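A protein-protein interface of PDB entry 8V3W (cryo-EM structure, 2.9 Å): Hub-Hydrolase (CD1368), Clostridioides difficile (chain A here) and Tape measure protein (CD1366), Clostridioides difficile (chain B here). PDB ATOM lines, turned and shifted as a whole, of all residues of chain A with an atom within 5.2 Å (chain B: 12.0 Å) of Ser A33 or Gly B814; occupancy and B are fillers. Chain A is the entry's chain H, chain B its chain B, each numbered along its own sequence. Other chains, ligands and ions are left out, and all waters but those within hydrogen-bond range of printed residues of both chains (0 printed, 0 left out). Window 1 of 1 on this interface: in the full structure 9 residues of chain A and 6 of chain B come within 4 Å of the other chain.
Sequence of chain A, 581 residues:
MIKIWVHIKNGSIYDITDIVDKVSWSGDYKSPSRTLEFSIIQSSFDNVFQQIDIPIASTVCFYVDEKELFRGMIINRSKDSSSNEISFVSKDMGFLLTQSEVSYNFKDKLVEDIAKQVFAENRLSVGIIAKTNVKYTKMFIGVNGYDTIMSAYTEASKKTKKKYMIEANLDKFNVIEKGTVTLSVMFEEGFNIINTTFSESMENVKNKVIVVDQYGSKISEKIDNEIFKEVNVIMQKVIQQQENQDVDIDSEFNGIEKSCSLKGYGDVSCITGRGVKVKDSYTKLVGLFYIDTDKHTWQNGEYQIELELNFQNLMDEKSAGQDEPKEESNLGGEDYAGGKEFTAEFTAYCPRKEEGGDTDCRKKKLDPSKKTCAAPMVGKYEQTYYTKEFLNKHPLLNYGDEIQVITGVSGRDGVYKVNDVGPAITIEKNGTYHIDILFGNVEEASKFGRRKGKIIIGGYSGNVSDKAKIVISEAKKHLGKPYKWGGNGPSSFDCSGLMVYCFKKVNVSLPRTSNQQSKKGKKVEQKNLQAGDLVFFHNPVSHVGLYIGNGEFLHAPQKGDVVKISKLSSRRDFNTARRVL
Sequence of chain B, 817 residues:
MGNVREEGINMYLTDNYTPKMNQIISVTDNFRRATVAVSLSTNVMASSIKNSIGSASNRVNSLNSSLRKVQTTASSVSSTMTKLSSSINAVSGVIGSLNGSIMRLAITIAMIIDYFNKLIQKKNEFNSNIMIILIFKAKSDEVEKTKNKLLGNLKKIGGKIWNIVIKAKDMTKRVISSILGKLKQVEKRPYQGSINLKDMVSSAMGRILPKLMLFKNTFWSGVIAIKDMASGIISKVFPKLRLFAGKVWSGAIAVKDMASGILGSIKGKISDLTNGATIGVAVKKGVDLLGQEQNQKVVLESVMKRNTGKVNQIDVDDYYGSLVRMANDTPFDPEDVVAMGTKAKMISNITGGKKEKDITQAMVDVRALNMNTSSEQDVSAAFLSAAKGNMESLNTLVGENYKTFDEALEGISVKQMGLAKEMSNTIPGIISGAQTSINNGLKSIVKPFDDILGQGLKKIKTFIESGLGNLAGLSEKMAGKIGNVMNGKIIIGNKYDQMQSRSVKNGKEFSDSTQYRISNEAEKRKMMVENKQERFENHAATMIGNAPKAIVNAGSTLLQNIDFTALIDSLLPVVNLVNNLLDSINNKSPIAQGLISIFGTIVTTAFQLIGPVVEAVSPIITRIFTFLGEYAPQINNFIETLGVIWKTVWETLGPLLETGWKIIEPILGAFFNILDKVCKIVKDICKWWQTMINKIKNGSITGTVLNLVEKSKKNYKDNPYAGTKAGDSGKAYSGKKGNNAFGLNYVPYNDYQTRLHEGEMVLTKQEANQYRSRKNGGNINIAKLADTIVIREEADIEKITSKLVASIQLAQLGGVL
The backbone carbonyl oxygen of Gly B814 lies within hydrogen-bond range of the side-chain hydroxyl of Ser A33 (3.3 Å).
No residue of chain B comes within 4 Å of Gly A27.
Ser A31 touches one residue of chain B.
Pro A32 touches just these residues of chain B: Gly B814 (3.9 Å) and Gly B815 (3.7 Å).
Ser A33 touches just one residue of chain B: Gly B814.
No residue of chain B comes within 4 Å of Thr A35.
No residue of chain B comes within 4 Å of Asp A92.
Printed residues of chain A within 4 Å of Leu B810: Lys A91 (3.9 Å).
Printed residues of chain A within 4 Å of Leu B813: Phe A95 (3.9 Å).
Gly B814 touches just these residues of chain A: Pro A32 (3.9 Å) and Ser A33 (3.3 Å).
Of the printed residues of chain A, Gly B815 touches Ser A31 (3.2 Å) and Pro A32 (3.7 Å).
Val B816 touches none of the printed residues of chain A.
The nearest residue of chain B that does not touch Ser A33 is Gly B815 (5.3 Å).
Ser A31 touches Gly B815 (CB to O, 3.2 Å).
O of Gly B814 touches CD of Pro A32 (3.9 Å).
Gly B815 touches Pro A32 (O to CD, 3.7 Å).
Leu B810 touches Lys A91 (CD1 to CE, 3.9 Å).
O of Leu B813 touches CB of Phe A95 (3.9 Å).
The backbone carbonyl oxygen (O) of Ser A33 sits at hydrogen-bond distance from the side-chain hydroxyl (OG) of Ser A31 (3.4 Å).
The side-chain hydroxyl (OG1) of Thr A98 lies within hydrogen-bond range of the backbone carbonyl oxygen (O) of Phe A95 (3.3 Å).
Of the 13 printed residues of chain B, 4 touch a printed residue of chain A.
Hydrophobic or aromatic side chains of chain A that line the printed part of chain B: Pro A32 and Phe A95.
Among the printed residues, 6 pairs touch across the chains.
Among the printed residues, no Asp or Glu carboxylate lies within 4 Å of a Lys or Arg side-chain nitrogen of the other chain.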
ATOM      1  N   GLY A  27      -8.330 -17.545  15.927  1.00  0.00           N
ATOM      2  CA  GLY A  27      -7.886 -17.665  17.302  1.00  0.00           C
ATOM      3  C   GLY A  27      -8.687 -18.724  18.024  1.00  0.00           C
ATOM      4  O   GLY A  27      -9.743 -19.158  17.556  1.00  0.00           O
ATOM      5  N   SER A  31      -5.328 -20.911  23.702  1.00  0.00           N
ATOM      6  CA  SER A  31      -4.017 -20.345  23.442  1.00  0.00           C
ATOM      7  C   SER A  31      -4.068 -18.837  23.625  1.00  0.00           C
ATOM      8  O   SER A  31      -5.100 -18.214  23.366  1.00  0.00           O
ATOM      9  CB  SER A  31      -3.539 -20.682  22.022  1.00  0.00           C
ATOM     10  OG  SER A  31      -4.307 -20.004  21.051  1.00  0.00           O
ATOM     11  N   PRO A  32      -2.974 -18.224  24.084  1.00  0.00           N
ATOM     12  CA  PRO A  32      -2.985 -16.775  24.323  1.00  0.00           C
ATOM     13  C   PRO A  32      -2.722 -15.921  23.092  1.00  0.00           C
ATOM     14  O   PRO A  32      -2.854 -14.694  23.181  1.00  0.00           O
ATOM     15  CB  PRO A  32      -1.867 -16.590  25.353  1.00  0.00           C
ATOM     16  CG  PRO A  32      -0.922 -17.690  25.055  1.00  0.00           C
ATOM     17  CD  PRO A  32      -1.756 -18.858  24.618  1.00  0.00           C
ATOM     18  N   SER A  33      -2.362 -16.509  21.957  1.00  0.00           N
ATOM     19  CA  SER A  33      -1.969 -15.741  20.786  1.00  0.00           C
ATOM     20  C   SER A  33      -2.864 -16.063  19.599  1.00  0.00           C
ATOM     21  O   SER A  33      -3.324 -17.193  19.432  1.00  0.00           O
ATOM     22  CB  SER A  33      -0.507 -16.002  20.418  1.00  0.00           C
ATOM     23  OG  SER A  33      -0.263 -17.385  20.269  1.00  0.00           O
ATOM     24  N   ARG A  34      -3.113 -15.046  18.785  1.00  0.00           N
ATOM     25  CA  ARG A  34      -3.856 -15.174  17.543  1.00  0.00           C
ATOM     26  C   ARG A  34      -2.878 -15.303  16.384  1.00  0.00           C
ATOM     27  O   ARG A  34      -1.693 -14.996  16.509  1.00  0.00           O
ATOM     28  CB  ARG A  34      -4.771 -13.967  17.333  1.00  0.00           C
ATOM     29  CG  ARG A  34      -5.927 -13.888  18.307  1.00  0.00           C
ATOM     30  CD  ARG A  34      -6.977 -12.902  17.842  1.00  0.00           C
ATOM     31  NE  ARG A  34      -8.305 -13.502  17.846  1.00  0.00           N
ATOM     32  CZ  ARG A  34      -9.031 -13.730  16.762  1.00  0.00           C
ATOM     33  NH1 ARG A  34      -8.601 -13.398  15.560  1.00  0.00           N
ATOM     34  NH2 ARG A  34     -10.216 -14.311  16.886  1.00  0.00           N
ATOM     35  N   THR A  35      -3.383 -15.760  15.247  1.00  0.00           N
ATOM     36  CA  THR A  35      -2.532 -16.040  14.103  1.00  0.00           C
ATOM     37  C   THR A  35      -3.094 -15.394  12.847  1.00  0.00           C
ATOM     38  O   THR A  35      -4.303 -15.192  12.719  1.00  0.00           O
ATOM     39  CB  THR A  35      -2.367 -17.552  13.895  1.00  0.00           C
ATOM     40  OG1 THR A  35      -1.679 -17.799  12.665  1.00  0.00           O
ATOM     41  CG2 THR A  35      -3.707 -18.231  13.858  1.00  0.00           C
ATOM     42  N   LYS A  91       2.340 -14.553  13.999  1.00  0.00           N
ATOM     43  CA  LYS A  91       1.803 -14.814  15.323  1.00  0.00           C
ATOM     44  C   LYS A  91       1.700 -13.527  16.122  1.00  0.00           C
ATOM     45  O   LYS A  91       2.506 -12.608  15.971  1.00  0.00           O
ATOM     46  CB  LYS A  91       2.657 -15.814  16.103  1.00  0.00           C
ATOM     47  CG  LYS A  91       2.376 -17.261  15.783  1.00  0.00           C
ATOM     48  CD  LYS A  91       1.072 -17.728  16.378  1.00  0.00           C
ATOM     49  CE  LYS A  91       0.920 -19.225  16.216  1.00  0.00           C
ATOM     50  NZ  LYS A  91      -0.380 -19.712  16.730  1.00  0.00           N
ATOM     51  N   ASP A  92       0.700 -13.491  16.992  1.00  0.00           N
ATOM     52  CA  ASP A  92       0.487 -12.386  17.908  1.00  0.00           C
ATOM     53  C   ASP A  92       1.668 -12.261  18.867  1.00  0.00           C
ATOM     54  O   ASP A  92       2.575 -13.088  18.890  1.00  0.00           O
ATOM     55  CB  ASP A  92      -0.801 -12.611  18.692  1.00  0.00           C
ATOM     56  CG  ASP A  92      -1.598 -11.362  18.860  1.00  0.00           C
ATOM     57  OD1 ASP A  92      -1.175 -10.320  18.327  1.00  0.00           O
ATOM     58  OD2 ASP A  92      -2.661 -11.428  19.508  1.00  0.00           O
ATOM     59  N   GLY A  94       1.319 -12.576  22.000  1.00  0.00           N
ATOM     60  CA  GLY A  94       0.975 -13.328  23.194  1.00  0.00           C
ATOM     61  C   GLY A  94       1.861 -14.521  23.483  1.00  0.00           C
ATOM     62  O   GLY A  94       1.851 -15.024  24.609  1.00  0.00           O
ATOM     63  N   PHE A  95       2.636 -14.987  22.504  1.00  0.00           N
ATOM     64  CA  PHE A  95       3.488 -16.145  22.748  1.00  0.00           C
ATOM     65  C   PHE A  95       4.709 -15.812  23.593  1.00  0.00           C
ATOM     66  O   PHE A  95       5.433 -16.729  23.987  1.00  0.00           O
ATOM     67  CB  PHE A  95       3.908 -16.787  21.420  1.00  0.00           C
ATOM     68  CG  PHE A  95       5.014 -16.070  20.703  1.00  0.00           C
ATOM     69  CD1 PHE A  95       4.732 -15.042  19.827  1.00  0.00           C
ATOM     70  CD2 PHE A  95       6.332 -16.448  20.873  1.00  0.00           C
ATOM     71  CE1 PHE A  95       5.740 -14.386  19.158  1.00  0.00           C
ATOM     72  CE2 PHE A  95       7.346 -15.795  20.203  1.00  0.00           C
ATOM     73  CZ  PHE A  95       7.048 -14.765  19.346  1.00  0.00           C
ATOM     74  N   THR A  98       4.636 -17.520  27.342  1.00  0.00           N
ATOM     75  CA  THR A  98       5.042 -18.898  27.585  1.00  0.00           C
ATOM     76  C   THR A  98       6.553 -19.088  27.562  1.00  0.00           C
ATOM     77  O   THR A  98       7.026 -20.161  27.944  1.00  0.00           O
ATOM     78  CB  THR A  98       4.395 -19.832  26.562  1.00  0.00           C
ATOM     79  OG1 THR A  98       5.126 -19.780  25.333  1.00  0.00           O
ATOM     80  CG2 THR A  98       2.959 -19.424  26.302  1.00  0.00           C
ATOM     81  N   VAL B 805       2.339 -32.764  11.570  1.00  0.00           N
ATOM     82  CA  VAL B 805       3.528 -32.394  12.334  1.00  0.00           C
ATOM     83  C   VAL B 805       3.751 -30.886  12.291  1.00  0.00           C
ATOM     84  O   VAL B 805       4.053 -30.261  13.315  1.00  0.00           O
ATOM     85  CB  VAL B 805       4.753 -33.169  11.817  1.00  0.00           C
ATOM     86  CG1 VAL B 805       6.037 -32.541  12.319  1.00  0.00           C
ATOM     87  CG2 VAL B 805       4.676 -34.616  12.248  1.00  0.00           C
ATOM     88  N   ALA B 806       3.607 -30.278  11.109  1.00  0.00           N
ATOM     89  CA  ALA B 806       3.788 -28.831  11.011  1.00  0.00           C
ATOM     90  C   ALA B 806       2.773 -28.083  11.870  1.00  0.00           C
ATOM     91  O   ALA B 806       3.125 -27.124  12.576  1.00  0.00           O
ATOM     92  CB  ALA B 806       3.688 -28.387   9.556  1.00  0.00           C
ATOM     93  N   SER B 807       1.511 -28.514  11.832  1.00  0.00           N
ATOM     94  CA  SER B 807       0.484 -27.861  12.638  1.00  0.00           C
ATOM     95  C   SER B 807       0.781 -27.990  14.127  1.00  0.00           C
ATOM     96  O   SER B 807       0.644 -27.018  14.883  1.00  0.00           O
ATOM     97  CB  SER B 807      -0.884 -28.450  12.310  1.00  0.00           C
ATOM     98  OG  SER B 807      -1.171 -28.312  10.932  1.00  0.00           O
ATOM     99  N   ILE B 808       1.201 -29.178  14.564  1.00  0.00           N
ATOM    100  CA  ILE B 808       1.491 -29.384  15.979  1.00  0.00           C
ATOM    101  C   ILE B 808       2.662 -28.516  16.419  1.00  0.00           C
ATOM    102  O   ILE B 808       2.650 -27.952  17.517  1.00  0.00           O
ATOM    103  CB  ILE B 808       1.752 -30.873  16.263  1.00  0.00           C
ATOM    104  CG1 ILE B 808       0.476 -31.684  16.061  1.00  0.00           C
ATOM    105  CG2 ILE B 808       2.264 -31.065  17.673  1.00  0.00           C
ATOM    106  CD1 ILE B 808       0.633 -33.144  16.370  1.00  0.00           C
ATOM    107  N   GLN B 809       3.694 -28.398  15.580  1.00  0.00           N
ATOM    108  CA  GLN B 809       4.843 -27.574  15.950  1.00  0.00           C
ATOM    109  C   GLN B 809       4.462 -26.101  16.064  1.00  0.00           C
ATOM    110  O   GLN B 809       4.893 -25.408  16.998  1.00  0.00           O
ATOM    111  CB  GLN B 809       5.972 -27.764  14.942  1.00  0.00           C
ATOM    112  CG  GLN B 809       6.794 -29.009  15.189  1.00  0.00           C
ATOM    113  CD  GLN B 809       7.542 -29.459  13.960  1.00  0.00           C
ATOM    114  OE1 GLN B 809       7.153 -29.145  12.837  1.00  0.00           O
ATOM    115  NE2 GLN B 809       8.610 -30.218  14.160  1.00  0.00           N
ATOM    116  N   LEU B 810       3.651 -25.604  15.126  1.00  0.00           N
ATOM    117  CA  LEU B 810       3.188 -24.223  15.230  1.00  0.00           C
ATOM    118  C   LEU B 810       2.393 -24.005  16.512  1.00  0.00           C
ATOM    119  O   LEU B 810       2.590 -23.004  17.214  1.00  0.00           O
ATOM    120  CB  LEU B 810       2.346 -23.855  14.012  1.00  0.00           C
ATOM    121  CG  LEU B 810       1.917 -22.390  13.920  1.00  0.00           C
ATOM    122  CD1 LEU B 810       3.120 -21.472  13.836  1.00  0.00           C
ATOM    123  CD2 LEU B 810       0.984 -22.172  12.741  1.00  0.00           C
ATOM    124  N   ALA B 811       1.503 -24.943  16.845  1.00  0.00           N
ATOM    125  CA  ALA B 811       0.708 -24.808  18.060  1.00  0.00           C
ATOM    126  C   ALA B 811       1.582 -24.850  19.307  1.00  0.00           C
ATOM    127  O   ALA B 811       1.315 -24.143  20.283  1.00  0.00           O
ATOM    128  CB  ALA B 811      -0.359 -25.898  18.114  1.00  0.00           C
ATOM    129  N   GLN B 812       2.626 -25.682  19.300  1.00  0.00           N
ATOM    130  CA  GLN B 812       3.546 -25.719  20.432  1.00  0.00           C
ATOM    131  C   GLN B 812       4.251 -24.384  20.609  1.00  0.00           C
ATOM    132  O   GLN B 812       4.432 -23.916  21.736  1.00  0.00           O
ATOM    133  CB  GLN B 812       4.579 -26.828  20.247  1.00  0.00           C
ATOM    134  CG  GLN B 812       4.086 -28.225  20.517  1.00  0.00           C
ATOM    135  CD  GLN B 812       5.177 -29.248  20.308  1.00  0.00           C
ATOM    136  OE1 GLN B 812       6.032 -29.087  19.440  1.00  0.00           O
ATOM    137  NE2 GLN B 812       5.161 -30.302  21.108  1.00  0.00           N
ATOM    138  N   LEU B 813       4.684 -23.770  19.503  1.00  0.00           N
ATOM    139  CA  LEU B 813       5.313 -22.457  19.606  1.00  0.00           C
ATOM    140  C   LEU B 813       4.337 -21.428  20.161  1.00  0.00           C
ATOM    141  O   LEU B 813       4.703 -20.609  21.010  1.00  0.00           O
ATOM    142  CB  LEU B 813       5.849 -22.016  18.242  1.00  0.00           C
ATOM    143  CG  LEU B 813       6.627 -20.699  18.088  1.00  0.00           C
ATOM    144  CD1 LEU B 813       5.706 -19.524  17.822  1.00  0.00           C
ATOM    145  CD2 LEU B 813       7.523 -20.410  19.281  1.00  0.00           C
ATOM    146  N   GLY B 814       3.085 -21.461  19.701  1.00  0.00           N
ATOM    147  CA  GLY B 814       2.108 -20.488  20.159  1.00  0.00           C
ATOM    148  C   GLY B 814       1.702 -20.637  21.611  1.00  0.00           C
ATOM    149  O   GLY B 814       1.206 -19.676  22.204  1.00  0.00           O
ATOM    150  N   GLY B 815       1.893 -21.817  22.193  1.00  0.00           N
ATOM    151  CA  GLY B 815       1.480 -22.071  23.559  1.00  0.00           C
ATOM    152  C   GLY B 815       0.087 -22.655  23.643  1.00  0.00           C
ATOM    153  O   GLY B 815      -0.851 -22.106  23.064  1.00  0.00           O
ATOM    154  N   VAL B 816      -0.065 -23.774  24.345  1.00  0.00           N
ATOM    155  CA  VAL B 816      -1.350 -24.445  24.495  1.00  0.00           C
ATOM    156  C   VAL B 816      -1.616 -24.636  25.979  1.00  0.00           C
ATOM    157  O   VAL B 816      -0.752 -25.130  26.711  1.00  0.00           O
ATOM    158  CB  VAL B 816      -1.381 -25.794  23.756  1.00  0.00           C
ATOM    159  CG1 VAL B 816      -2.654 -26.546  24.075  1.00  0.00           C
ATOM    160  CG2 VAL B 816      -1.260 -25.584  22.262  1.00  0.00           C
ATOM    161  N   LEU B 817      -2.803 -24.245  26.420  1.00  0.00           N
ATOM    162  CA  LEU B 817      -3.180 -24.390  27.816  1.00  0.00           C
ATOM    163  C   LEU B 817      -3.440 -25.848  28.165  1.00  0.00           C
ATOM    164  O   LEU B 817      -2.508 -26.624  28.368  1.00  0.00           O
ATOM    165  CB  LEU B 817      -4.420 -23.559  28.124  1.00  0.00           C
ATOM    166  CG  LEU B 817      -5.023 -23.780  29.507  1.00  0.00           C
ATOM    167  CD1 LEU B 817      -4.146 -23.134  30.561  1.00  0.00           C
ATOM    168  CD2 LEU B 817      -6.434 -23.235  29.567  1.00  0.00           C
